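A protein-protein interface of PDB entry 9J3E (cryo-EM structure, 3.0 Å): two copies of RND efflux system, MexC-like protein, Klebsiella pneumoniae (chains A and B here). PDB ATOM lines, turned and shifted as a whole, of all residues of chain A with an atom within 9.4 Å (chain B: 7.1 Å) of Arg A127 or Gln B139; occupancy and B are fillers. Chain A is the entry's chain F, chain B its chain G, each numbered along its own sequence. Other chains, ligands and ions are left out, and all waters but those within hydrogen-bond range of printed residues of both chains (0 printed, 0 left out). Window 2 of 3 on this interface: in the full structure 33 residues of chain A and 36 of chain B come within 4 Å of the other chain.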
ATOM      1  N   LEU A 118      29.554 -18.499  26.983  1.00  0.00           N
ATOM      2  CA  LEU A 118      28.822 -17.365  26.432  1.00  0.00           C
ATOM      3  C   LEU A 118      27.509 -17.805  25.812  1.00  0.00           C
ATOM      4  O   LEU A 118      26.487 -17.132  25.968  1.00  0.00           O
ATOM      5  CB  LEU A 118      29.671 -16.645  25.391  1.00  0.00           C
ATOM      6  CG  LEU A 118      28.900 -15.660  24.516  1.00  0.00           C
ATOM      7  CD1 LEU A 118      28.343 -14.524  25.342  1.00  0.00           C
ATOM      8  CD2 LEU A 118      29.776 -15.134  23.406  1.00  0.00           C
ATOM      9  N   PHE A 119      27.520 -18.920  25.086  1.00  0.00           N
ATOM     10  CA  PHE A 119      26.292 -19.419  24.484  1.00  0.00           C
ATOM     11  C   PHE A 119      25.266 -19.751  25.553  1.00  0.00           C
ATOM     12  O   PHE A 119      24.083 -19.406  25.428  1.00  0.00           O
ATOM     13  CB  PHE A 119      26.596 -20.652  23.641  1.00  0.00           C
ATOM     14  CG  PHE A 119      25.380 -21.314  23.085  1.00  0.00           C
ATOM     15  CD1 PHE A 119      24.778 -20.826  21.943  1.00  0.00           C
ATOM     16  CD2 PHE A 119      24.827 -22.413  23.712  1.00  0.00           C
ATOM     17  CE1 PHE A 119      23.655 -21.428  21.427  1.00  0.00           C
ATOM     18  CE2 PHE A 119      23.702 -23.017  23.204  1.00  0.00           C
ATOM     19  CZ  PHE A 119      23.115 -22.524  22.058  1.00  0.00           C
ATOM     20  N   GLN A 120      25.708 -20.413  26.621  1.00  0.00           N
ATOM     21  CA  GLN A 120      24.796 -20.750  27.705  1.00  0.00           C
ATOM     22  C   GLN A 120      24.207 -19.495  28.335  1.00  0.00           C
ATOM     23  O   GLN A 120      23.000 -19.421  28.594  1.00  0.00           O
ATOM     24  CB  GLN A 120      25.526 -21.591  28.746  1.00  0.00           C
ATOM     25  CG  GLN A 120      24.638 -22.147  29.827  1.00  0.00           C
ATOM     26  CD  GLN A 120      24.521 -21.215  31.002  1.00  0.00           C
ATOM     27  OE1 GLN A 120      25.178 -20.180  31.052  1.00  0.00           O
ATOM     28  NE2 GLN A 120      23.677 -21.574  31.958  1.00  0.00           N
ATOM     29  N   ALA A 121      25.048 -18.493  28.588  1.00  0.00           N
ATOM     30  CA  ALA A 121      24.558 -17.264  29.204  1.00  0.00           C
ATOM     31  C   ALA A 121      23.594 -16.528  28.286  1.00  0.00           C
ATOM     32  O   ALA A 121      22.597 -15.960  28.746  1.00  0.00           O
ATOM     33  CB  ALA A 121      25.730 -16.363  29.581  1.00  0.00           C
ATOM     34  N   GLN A 122      23.881 -16.517  26.985  1.00  0.00           N
ATOM     35  CA  GLN A 122      22.971 -15.895  26.033  1.00  0.00           C
ATOM     36  C   GLN A 122      21.618 -16.578  26.052  1.00  0.00           C
ATOM     37  O   GLN A 122      20.579 -15.913  26.026  1.00  0.00           O
ATOM     38  CB  GLN A 122      23.557 -15.950  24.625  1.00  0.00           C
ATOM     39  CG  GLN A 122      24.575 -14.885  24.316  1.00  0.00           C
ATOM     40  CD  GLN A 122      25.147 -15.035  22.924  1.00  0.00           C
ATOM     41  OE1 GLN A 122      24.898 -16.029  22.245  1.00  0.00           O
ATOM     42  NE2 GLN A 122      25.908 -14.041  22.487  1.00  0.00           N
ATOM     43  N   ALA A 123      21.609 -17.911  26.087  1.00  0.00           N
ATOM     44  CA  ALA A 123      20.340 -18.627  26.154  1.00  0.00           C
ATOM     45  C   ALA A 123      19.594 -18.295  27.438  1.00  0.00           C
ATOM     46  O   ALA A 123      18.375 -18.083  27.423  1.00  0.00           O
ATOM     47  CB  ALA A 123      20.576 -20.130  26.043  1.00  0.00           C
ATOM     48  N   MET A 124      20.314 -18.240  28.559  1.00  0.00           N
ATOM     49  CA  MET A 124      19.691 -17.877  29.828  1.00  0.00           C
ATOM     50  C   MET A 124      19.019 -16.516  29.741  1.00  0.00           C
ATOM     51  O   MET A 124      17.866 -16.351  30.151  1.00  0.00           O
ATOM     52  CB  MET A 124      20.735 -17.873  30.939  1.00  0.00           C
ATOM     53  CG  MET A 124      20.242 -17.280  32.237  1.00  0.00           C
ATOM     54  SD  MET A 124      20.701 -18.250  33.673  1.00  0.00           S
ATOM     55  CE  MET A 124      19.491 -19.554  33.578  1.00  0.00           C
ATOM     56  N   VAL A 125      19.731 -15.525  29.213  1.00  0.00           N
ATOM     57  CA  VAL A 125      19.175 -14.180  29.160  1.00  0.00           C
ATOM     58  C   VAL A 125      18.014 -14.122  28.179  1.00  0.00           C
ATOM     59  O   VAL A 125      17.015 -13.441  28.426  1.00  0.00           O
ATOM     60  CB  VAL A 125      20.270 -13.158  28.817  1.00  0.00           C
ATOM     61  CG1 VAL A 125      19.654 -11.859  28.352  1.00  0.00           C
ATOM     62  CG2 VAL A 125      21.143 -12.918  30.024  1.00  0.00           C
ATOM     63  N   ARG A 126      18.116 -14.838  27.060  1.00  0.00           N
ATOM     64  CA  ARG A 126      17.016 -14.847  26.104  1.00  0.00           C
ATOM     65  C   ARG A 126      15.762 -15.448  26.714  1.00  0.00           C
ATOM     66  O   ARG A 126      14.650 -15.007  26.415  1.00  0.00           O
ATOM     67  CB  ARG A 126      17.404 -15.607  24.839  1.00  0.00           C
ATOM     68  CG  ARG A 126      18.144 -14.769  23.824  1.00  0.00           C
ATOM     69  CD  ARG A 126      18.198 -15.463  22.476  1.00  0.00           C
ATOM     70  NE  ARG A 126      18.850 -16.764  22.557  1.00  0.00           N
ATOM     71  CZ  ARG A 126      19.917 -17.106  21.851  1.00  0.00           C
ATOM     72  NH1 ARG A 126      20.477 -16.268  20.994  1.00  0.00           N
ATOM     73  NH2 ARG A 126      20.438 -18.320  22.008  1.00  0.00           N
ATOM     74  N   ARG A 127      15.914 -16.467  27.557  1.00  0.00           N
ATOM     75  CA  ARG A 127      14.733 -17.039  28.191  1.00  0.00           C
ATOM     76  C   ARG A 127      14.202 -16.136  29.293  1.00  0.00           C
ATOM     77  O   ARG A 127      12.987 -16.013  29.463  1.00  0.00           O
ATOM     78  CB  ARG A 127      15.038 -18.426  28.737  1.00  0.00           C
ATOM     79  CG  ARG A 127      14.935 -19.487  27.679  1.00  0.00           C
ATOM     80  CD  ARG A 127      15.374 -20.829  28.189  1.00  0.00           C
ATOM     81  NE  ARG A 127      16.820 -20.910  28.293  1.00  0.00           N
ATOM     82  CZ  ARG A 127      17.512 -22.020  28.092  1.00  0.00           C
ATOM     83  NH1 ARG A 127      16.919 -23.148  27.744  1.00  0.00           N
ATOM     84  NH2 ARG A 127      18.832 -21.996  28.242  1.00  0.00           N
ATOM     85  N   TYR A 128      15.090 -15.497  30.048  1.00  0.00           N
ATOM     86  CA  TYR A 128      14.654 -14.673  31.167  1.00  0.00           C
ATOM     87  C   TYR A 128      14.041 -13.354  30.727  1.00  0.00           C
ATOM     88  O   TYR A 128      13.207 -12.803  31.452  1.00  0.00           O
ATOM     89  CB  TYR A 128      15.829 -14.395  32.099  1.00  0.00           C
ATOM     90  CG  TYR A 128      16.028 -15.447  33.154  1.00  0.00           C
ATOM     91  CD1 TYR A 128      15.506 -16.716  32.998  1.00  0.00           C
ATOM     92  CD2 TYR A 128      16.755 -15.178  34.297  1.00  0.00           C
ATOM     93  CE1 TYR A 128      15.691 -17.683  33.956  1.00  0.00           C
ATOM     94  CE2 TYR A 128      16.946 -16.136  35.259  1.00  0.00           C
ATOM     95  CZ  TYR A 128      16.413 -17.387  35.085  1.00  0.00           C
ATOM     96  OH  TYR A 128      16.602 -18.346  36.048  1.00  0.00           O
ATOM     97  N   GLU A 129      14.429 -12.841  29.564  1.00  0.00           N
ATOM     98  CA  GLU A 129      13.974 -11.517  29.145  1.00  0.00           C
ATOM     99  C   GLU A 129      12.463 -11.423  28.995  1.00  0.00           C
ATOM    100  O   GLU A 129      11.880 -10.452  29.505  1.00  0.00           O
ATOM    101  CB  GLU A 129      14.702 -11.126  27.858  1.00  0.00           C
ATOM    102  CG  GLU A 129      14.631  -9.662  27.512  1.00  0.00           C
ATOM    103  CD  GLU A 129      15.180  -9.387  26.132  1.00  0.00           C
ATOM    104  OE1 GLU A 129      15.957 -10.225  25.631  1.00  0.00           O
ATOM    105  OE2 GLU A 129      14.837  -8.339  25.548  1.00  0.00           O
ATOM    106  N   PRO A 130      11.768 -12.349  28.328  1.00  0.00           N
ATOM    107  CA  PRO A 130      10.302 -12.266  28.318  1.00  0.00           C
ATOM    108  C   PRO A 130       9.683 -12.597  29.654  1.00  0.00           C
ATOM    109  O   PRO A 130       8.581 -12.118  29.942  1.00  0.00           O
ATOM    110  CB  PRO A 130       9.899 -13.288  27.250  1.00  0.00           C
ATOM    111  CG  PRO A 130      10.988 -14.264  27.256  1.00  0.00           C
ATOM    112  CD  PRO A 130      12.238 -13.477  27.509  1.00  0.00           C
ATOM    113  N   LEU A 131      10.355 -13.393  30.482  1.00  0.00           N
ATOM    114  CA  LEU A 131       9.762 -13.795  31.748  1.00  0.00           C
ATOM    115  C   LEU A 131       9.815 -12.677  32.778  1.00  0.00           C
ATOM    116  O   LEU A 131       8.875 -12.516  33.559  1.00  0.00           O
ATOM    117  CB  LEU A 131      10.465 -15.036  32.280  1.00  0.00           C
ATOM    118  CG  LEU A 131      10.267 -16.289  31.434  1.00  0.00           C
ATOM    119  CD1 LEU A 131      11.043 -17.445  32.017  1.00  0.00           C
ATOM    120  CD2 LEU A 131       8.800 -16.625  31.344  1.00  0.00           C
ATOM    121  N   VAL A 132      10.897 -11.900  32.801  1.00  0.00           N
ATOM    122  CA  VAL A 132      11.016 -10.862  33.817  1.00  0.00           C
ATOM    123  C   VAL A 132       9.995  -9.759  33.585  1.00  0.00           C
ATOM    124  O   VAL A 132       9.583  -9.076  34.529  1.00  0.00           O
ATOM    125  CB  VAL A 132      12.451 -10.312  33.859  1.00  0.00           C
ATOM    126  CG1 VAL A 132      12.738  -9.478  32.633  1.00  0.00           C
ATOM    127  CG2 VAL A 132      12.664  -9.501  35.114  1.00  0.00           C
ATOM    128  N   LYS A 133       9.565  -9.562  32.338  1.00  0.00           N
ATOM    129  CA  LYS A 133       8.565  -8.539  32.063  1.00  0.00           C
ATOM    130  C   LYS A 133       7.220  -8.884  32.682  1.00  0.00           C
ATOM    131  O   LYS A 133       6.492  -7.984  33.113  1.00  0.00           O
ATOM    132  CB  LYS A 133       8.424  -8.327  30.558  1.00  0.00           C
ATOM    133  CG  LYS A 133       9.301  -7.209  30.020  1.00  0.00           C
ATOM    134  CD  LYS A 133       9.155  -7.047  28.517  1.00  0.00           C
ATOM    135  CE  LYS A 133       9.193  -8.381  27.804  1.00  0.00           C
ATOM    136  NZ  LYS A 133      10.506  -9.045  28.012  1.00  0.00           N
ATOM    137  N   ILE A 134       6.870 -10.167  32.738  1.00  0.00           N
ATOM    138  CA  ILE A 134       5.669 -10.604  33.436  1.00  0.00           C
ATOM    139  C   ILE A 134       5.975 -11.027  34.864  1.00  0.00           C
ATOM    140  O   ILE A 134       5.146 -11.677  35.504  1.00  0.00           O
ATOM    141  CB  ILE A 134       4.961 -11.737  32.681  1.00  0.00           C
ATOM    142  CG1 ILE A 134       5.925 -12.889  32.438  1.00  0.00           C
ATOM    143  CG2 ILE A 134       4.418 -11.228  31.369  1.00  0.00           C
ATOM    144  CD1 ILE A 134       5.283 -14.076  31.795  1.00  0.00           C
ATOM    145  N   ALA A 136       7.764 -13.286  36.010  1.00  0.00           N
ATOM    146  CA  ALA A 136       7.892 -14.719  36.237  1.00  0.00           C
ATOM    147  C   ALA A 136       9.179 -15.052  36.973  1.00  0.00           C
ATOM    148  O   ALA A 136       9.204 -15.981  37.785  1.00  0.00           O
ATOM    149  CB  ALA A 136       7.830 -15.472  34.913  1.00  0.00           C
ATOM    150  N   VAL A 137      10.253 -14.311  36.707  1.00  0.00           N
ATOM    151  CA  VAL A 137      11.511 -14.474  37.415  1.00  0.00           C
ATOM    152  C   VAL A 137      11.816 -13.171  38.135  1.00  0.00           C
ATOM    153  O   VAL A 137      11.450 -12.084  37.685  1.00  0.00           O
ATOM    154  CB  VAL A 137      12.672 -14.854  36.479  1.00  0.00           C
ATOM    155  CG1 VAL A 137      12.404 -16.196  35.838  1.00  0.00           C
ATOM    156  CG2 VAL A 137      12.859 -13.792  35.424  1.00  0.00           C
ATOM    157  N   PHE A 142      17.130 -11.808  37.043  1.00  0.00           N
ATOM    158  CA  PHE A 142      17.413 -11.281  35.715  1.00  0.00           C
ATOM    159  C   PHE A 142      18.700 -10.477  35.704  1.00  0.00           C
ATOM    160  O   PHE A 142      19.477 -10.552  34.750  1.00  0.00           O
ATOM    161  CB  PHE A 142      16.265 -10.420  35.211  1.00  0.00           C
ATOM    162  CG  PHE A 142      16.503  -9.873  33.844  1.00  0.00           C
ATOM    163  CD1 PHE A 142      16.626 -10.722  32.764  1.00  0.00           C
ATOM    164  CD2 PHE A 142      16.637  -8.516  33.640  1.00  0.00           C
ATOM    165  CE1 PHE A 142      16.854 -10.229  31.506  1.00  0.00           C
ATOM    166  CE2 PHE A 142      16.866  -8.018  32.381  1.00  0.00           C
ATOM    167  CZ  PHE A 142      16.976  -8.876  31.314  1.00  0.00           C
ATOM    168  N   ALA A 145      21.493 -12.868  35.656  1.00  0.00           N
ATOM    169  CA  ALA A 145      21.671 -13.426  34.322  1.00  0.00           C
ATOM    170  C   ALA A 145      22.361 -12.435  33.398  1.00  0.00           C
ATOM    171  O   ALA A 145      23.218 -12.814  32.596  1.00  0.00           O
ATOM    172  CB  ALA A 145      20.323 -13.845  33.745  1.00  0.00           C
ATOM    173  N   VAL B 132      14.367 -34.081  27.774  1.00  0.00           N
ATOM    174  CA  VAL B 132      13.946 -32.743  27.395  1.00  0.00           C
ATOM    175  C   VAL B 132      12.944 -32.781  26.254  1.00  0.00           C
ATOM    176  O   VAL B 132      12.136 -31.859  26.115  1.00  0.00           O
ATOM    177  CB  VAL B 132      15.164 -31.877  27.032  1.00  0.00           C
ATOM    178  CG1 VAL B 132      15.704 -32.257  25.674  1.00  0.00           C
ATOM    179  CG2 VAL B 132      14.789 -30.417  27.060  1.00  0.00           C
ATOM    180  N   LYS B 133      12.964 -33.834  25.437  1.00  0.00           N
ATOM    181  CA  LYS B 133      11.992 -33.943  24.358  1.00  0.00           C
ATOM    182  C   LYS B 133      10.570 -34.062  24.881  1.00  0.00           C
ATOM    183  O   LYS B 133       9.637 -33.612  24.209  1.00  0.00           O
ATOM    184  CB  LYS B 133      12.320 -35.140  23.468  1.00  0.00           C
ATOM    185  CG  LYS B 133      12.893 -34.763  22.115  1.00  0.00           C
ATOM    186  CD  LYS B 133      13.140 -35.993  21.261  1.00  0.00           C
ATOM    187  CE  LYS B 133      14.592 -36.425  21.314  1.00  0.00           C
ATOM    188  NZ  LYS B 133      15.485 -35.426  20.664  1.00  0.00           N
ATOM    189  N   ASP B 135       9.846 -32.833  27.965  1.00  0.00           N
ATOM    190  CA  ASP B 135       9.856 -31.792  28.986  1.00  0.00           C
ATOM    191  C   ASP B 135      10.077 -32.335  30.389  1.00  0.00           C
ATOM    192  O   ASP B 135       9.776 -31.643  31.365  1.00  0.00           O
ATOM    193  CB  ASP B 135       8.567 -30.967  28.953  1.00  0.00           C
ATOM    194  CG  ASP B 135       8.799 -29.555  28.473  1.00  0.00           C
ATOM    195  OD1 ASP B 135       9.958 -29.220  28.162  1.00  0.00           O
ATOM    196  OD2 ASP B 135       7.823 -28.782  28.392  1.00  0.00           O
ATOM    197  N   VAL B 137      12.898 -32.691  31.789  1.00  0.00           N
ATOM    198  CA  VAL B 137      13.886 -31.773  32.329  1.00  0.00           C
ATOM    199  C   VAL B 137      13.702 -30.434  31.637  1.00  0.00           C
ATOM    200  O   VAL B 137      13.308 -30.357  30.473  1.00  0.00           O
ATOM    201  CB  VAL B 137      15.330 -32.275  32.150  1.00  0.00           C
ATOM    202  CG1 VAL B 137      15.542 -33.544  32.937  1.00  0.00           C
ATOM    203  CG2 VAL B 137      15.630 -32.502  30.689  1.00  0.00           C
ATOM    204  N   SER B 138      13.981 -29.368  32.376  1.00  0.00           N
ATOM    205  CA  SER B 138      13.822 -28.036  31.826  1.00  0.00           C
ATOM    206  C   SER B 138      14.760 -27.845  30.649  1.00  0.00           C
ATOM    207  O   SER B 138      15.870 -28.378  30.622  1.00  0.00           O
ATOM    208  CB  SER B 138      14.115 -26.980  32.885  1.00  0.00           C
ATOM    209  OG  SER B 138      15.507 -26.741  32.976  1.00  0.00           O
ATOM    210  N   GLN B 139      14.299 -27.085  29.657  1.00  0.00           N
ATOM    211  CA  GLN B 139      15.187 -26.723  28.562  1.00  0.00           C
ATOM    212  C   GLN B 139      16.420 -26.008  29.083  1.00  0.00           C
ATOM    213  O   GLN B 139      17.507 -26.145  28.513  1.00  0.00           O
ATOM    214  CB  GLN B 139      14.451 -25.851  27.551  1.00  0.00           C
ATOM    215  CG  GLN B 139      15.266 -25.530  26.317  1.00  0.00           C
ATOM    216  CD  GLN B 139      15.572 -26.758  25.490  1.00  0.00           C
ATOM    217  OE1 GLN B 139      14.733 -27.645  25.344  1.00  0.00           O
ATOM    218  NE2 GLN B 139      16.780 -26.818  24.943  1.00  0.00           N
ATOM    219  N   GLN B 140      16.274 -25.258  30.173  1.00  0.00           N
ATOM    220  CA  GLN B 140      17.425 -24.605  30.779  1.00  0.00           C
ATOM    221  C   GLN B 140      18.415 -25.628  31.311  1.00  0.00           C
ATOM    222  O   GLN B 140      19.629 -25.466  31.152  1.00  0.00           O
ATOM    223  CB  GLN B 140      16.971 -23.681  31.901  1.00  0.00           C
ATOM    224  CG  GLN B 140      18.110 -22.967  32.561  1.00  0.00           C
ATOM    225  CD  GLN B 140      18.894 -22.145  31.570  1.00  0.00           C
ATOM    226  OE1 GLN B 140      18.319 -21.391  30.790  1.00  0.00           O
ATOM    227  NE2 GLN B 140      20.214 -22.287  31.588  1.00  0.00           N
ATOM    228  N   ASP B 141      17.918 -26.683  31.956  1.00  0.00           N
ATOM    229  CA  ASP B 141      18.815 -27.710  32.476  1.00  0.00           C
ATOM    230  C   ASP B 141      19.551 -28.414  31.348  1.00  0.00           C
ATOM    231  O   ASP B 141      20.747 -28.698  31.460  1.00  0.00           O
ATOM    232  CB  ASP B 141      18.041 -28.721  33.316  1.00  0.00           C
ATOM    233  CG  ASP B 141      17.736 -28.210  34.706  1.00  0.00           C
ATOM    234  OD1 ASP B 141      18.635 -27.612  35.334  1.00  0.00           O
ATOM    235  OD2 ASP B 141      16.599 -28.415  35.179  1.00  0.00           O
ATOM    236  N   PHE B 142      18.854 -28.706  30.253  1.00  0.00           N
ATOM    237  CA  PHE B 142      19.517 -29.337  29.121  1.00  0.00           C
ATOM    238  C   PHE B 142      20.545 -28.405  28.500  1.00  0.00           C
ATOM    239  O   PHE B 142      21.600 -28.855  28.048  1.00  0.00           O
ATOM    240  CB  PHE B 142      18.503 -29.764  28.071  1.00  0.00           C
ATOM    241  CG  PHE B 142      19.128 -30.348  26.850  1.00  0.00           C
ATOM    242  CD1 PHE B 142      19.724 -31.588  26.896  1.00  0.00           C
ATOM    243  CD2 PHE B 142      19.149 -29.648  25.664  1.00  0.00           C
ATOM    244  CE1 PHE B 142      20.305 -32.129  25.780  1.00  0.00           C
ATOM    245  CE2 PHE B 142      19.733 -30.185  24.544  1.00  0.00           C
ATOM    246  CZ  PHE B 142      20.311 -31.428  24.603  1.00  0.00           C
ATOM    247  N   ASP B 143      20.246 -27.108  28.438  1.00  0.00           N
ATOM    248  CA  ASP B 143      21.228 -26.170  27.905  1.00  0.00           C
ATOM    249  C   ASP B 143      22.453 -26.092  28.800  1.00  0.00           C
ATOM    250  O   ASP B 143      23.582 -26.011  28.310  1.00  0.00           O
ATOM    251  CB  ASP B 143      20.607 -24.788  27.726  1.00  0.00           C
ATOM    252  CG  ASP B 143      19.762 -24.696  26.479  1.00  0.00           C
ATOM    253  OD1 ASP B 143      19.747 -25.670  25.703  1.00  0.00           O
ATOM    254  OD2 ASP B 143      19.129 -23.645  26.259  1.00  0.00           O
ATOM    255  N   ASN B 144      22.252 -26.124  30.115  1.00  0.00           N
ATOM    256  CA  ASN B 144      23.386 -26.167  31.026  1.00  0.00           C
ATOM    257  C   ASN B 144      24.192 -27.441  30.827  1.00  0.00           C
ATOM    258  O   ASN B 144      25.425 -27.414  30.860  1.00  0.00           O
ATOM    259  CB  ASN B 144      22.909 -26.060  32.470  1.00  0.00           C
ATOM    260  CG  ASN B 144      22.398 -24.682  32.808  1.00  0.00           C
ATOM    261  OD1 ASN B 144      22.653 -23.721  32.088  1.00  0.00           O
ATOM    262  ND2 ASN B 144      21.674 -24.576  33.912  1.00  0.00           N
ATOM    263  N   ALA B 145      23.511 -28.566  30.620  1.00  0.00           N
ATOM    264  CA  ALA B 145      24.216 -29.821  30.383  1.00  0.00           C
ATOM    265  C   ALA B 145      25.012 -29.768  29.090  1.00  0.00           C
ATOM    266  O   ALA B 145      26.149 -30.244  29.033  1.00  0.00           O
ATOM    267  CB  ALA B 145      23.225 -30.979  30.353  1.00  0.00           C
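Positions printed for both chains: 132, 133, 137, 142 and 145.
Of the 7 pairs that touch across the chains among the printed residues, none has its exchanged pair printed and touching as well.
NH2 of Arg A127 is in hydrogen-bond range of OE1 of Gln B140, 2.7 Å away.
NE2 of Gln A120 sits close to OD1 of Asn B144, at 2.4 Å.
The side-chain carboxylate (OD2) of Asp B143 is in salt-bridge range of the guanidinium group (NH2) of Arg A127 (2.6 Å).
The guanidinium group (NH1) of Arg A127 lies within hydrogen-bond range of the backbone carbonyl oxygen (O) of Gln B139.
OG of Ser B138 lies close to N of Gln B140, at 3.3 Å.
The side-chain amide nitrogen (NE2) of Gln B139 sits at hydrogen-bond distance from the side-chain carboxylate (OD1) of Asp B143 (3.3 Å).
O of Ala A123 is in hydrogen-bond range of NE of Arg A127.
The side-chain amide nitrogen (NE2) of Gln B140 lies within hydrogen-bond range of the side-chain amide oxygen (OD1) of Asn B144, 2.9 Å away.
Of chain B, only Gln B139 (3.1 Å), Gln B140 (2.7 Å) and Asp B143 (2.6 Å) come within 4 Å of Arg A127.
Gln B139 touches just one residue of chain A: Arg A127.
Ser B138 touches none of the printed residues of chain A.
Of the printed residues of chain A, Asn B144 touches Gln A120.
Printed residues of chain B within 4 Å of Gln A120: Gln B140 (3.6 Å) and Asn B144 (2.4 Å).
Of the printed residues of chain A, Asp B143 touches Ala A123 and Arg A127.
Of the printed residues of chain B, Ala A123 touches Asp B143.
Of the printed residues of chain B, Met A124 touches Gln B140.
The nearest residue of chain A that does not touch Gln B139 is Ala A123 (7.2 Å).
The nearest printed residue of chain B that does not touch Ala A123 is Gln B140 (4.7 Å).
Hydrophobic or aromatic side chains of chain A that line the printed part of chain B: Ala A123 and Met A124.
Of the 12 printed residues of chain B, 4 touch a printed residue of chain A.
Among the printed residues, Asp or Glu carboxylates within 4 Å of a Lys or Arg side-chain nitrogen of the other chain: Arg A127 with Asp B143.
Gln B140 touches Gln A120.
OD2 of Asp B143 touches CB of Ala A123, at 3.8 Å.
Met A124 touches Gln B140 (CE to CD, 3.3 Å).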
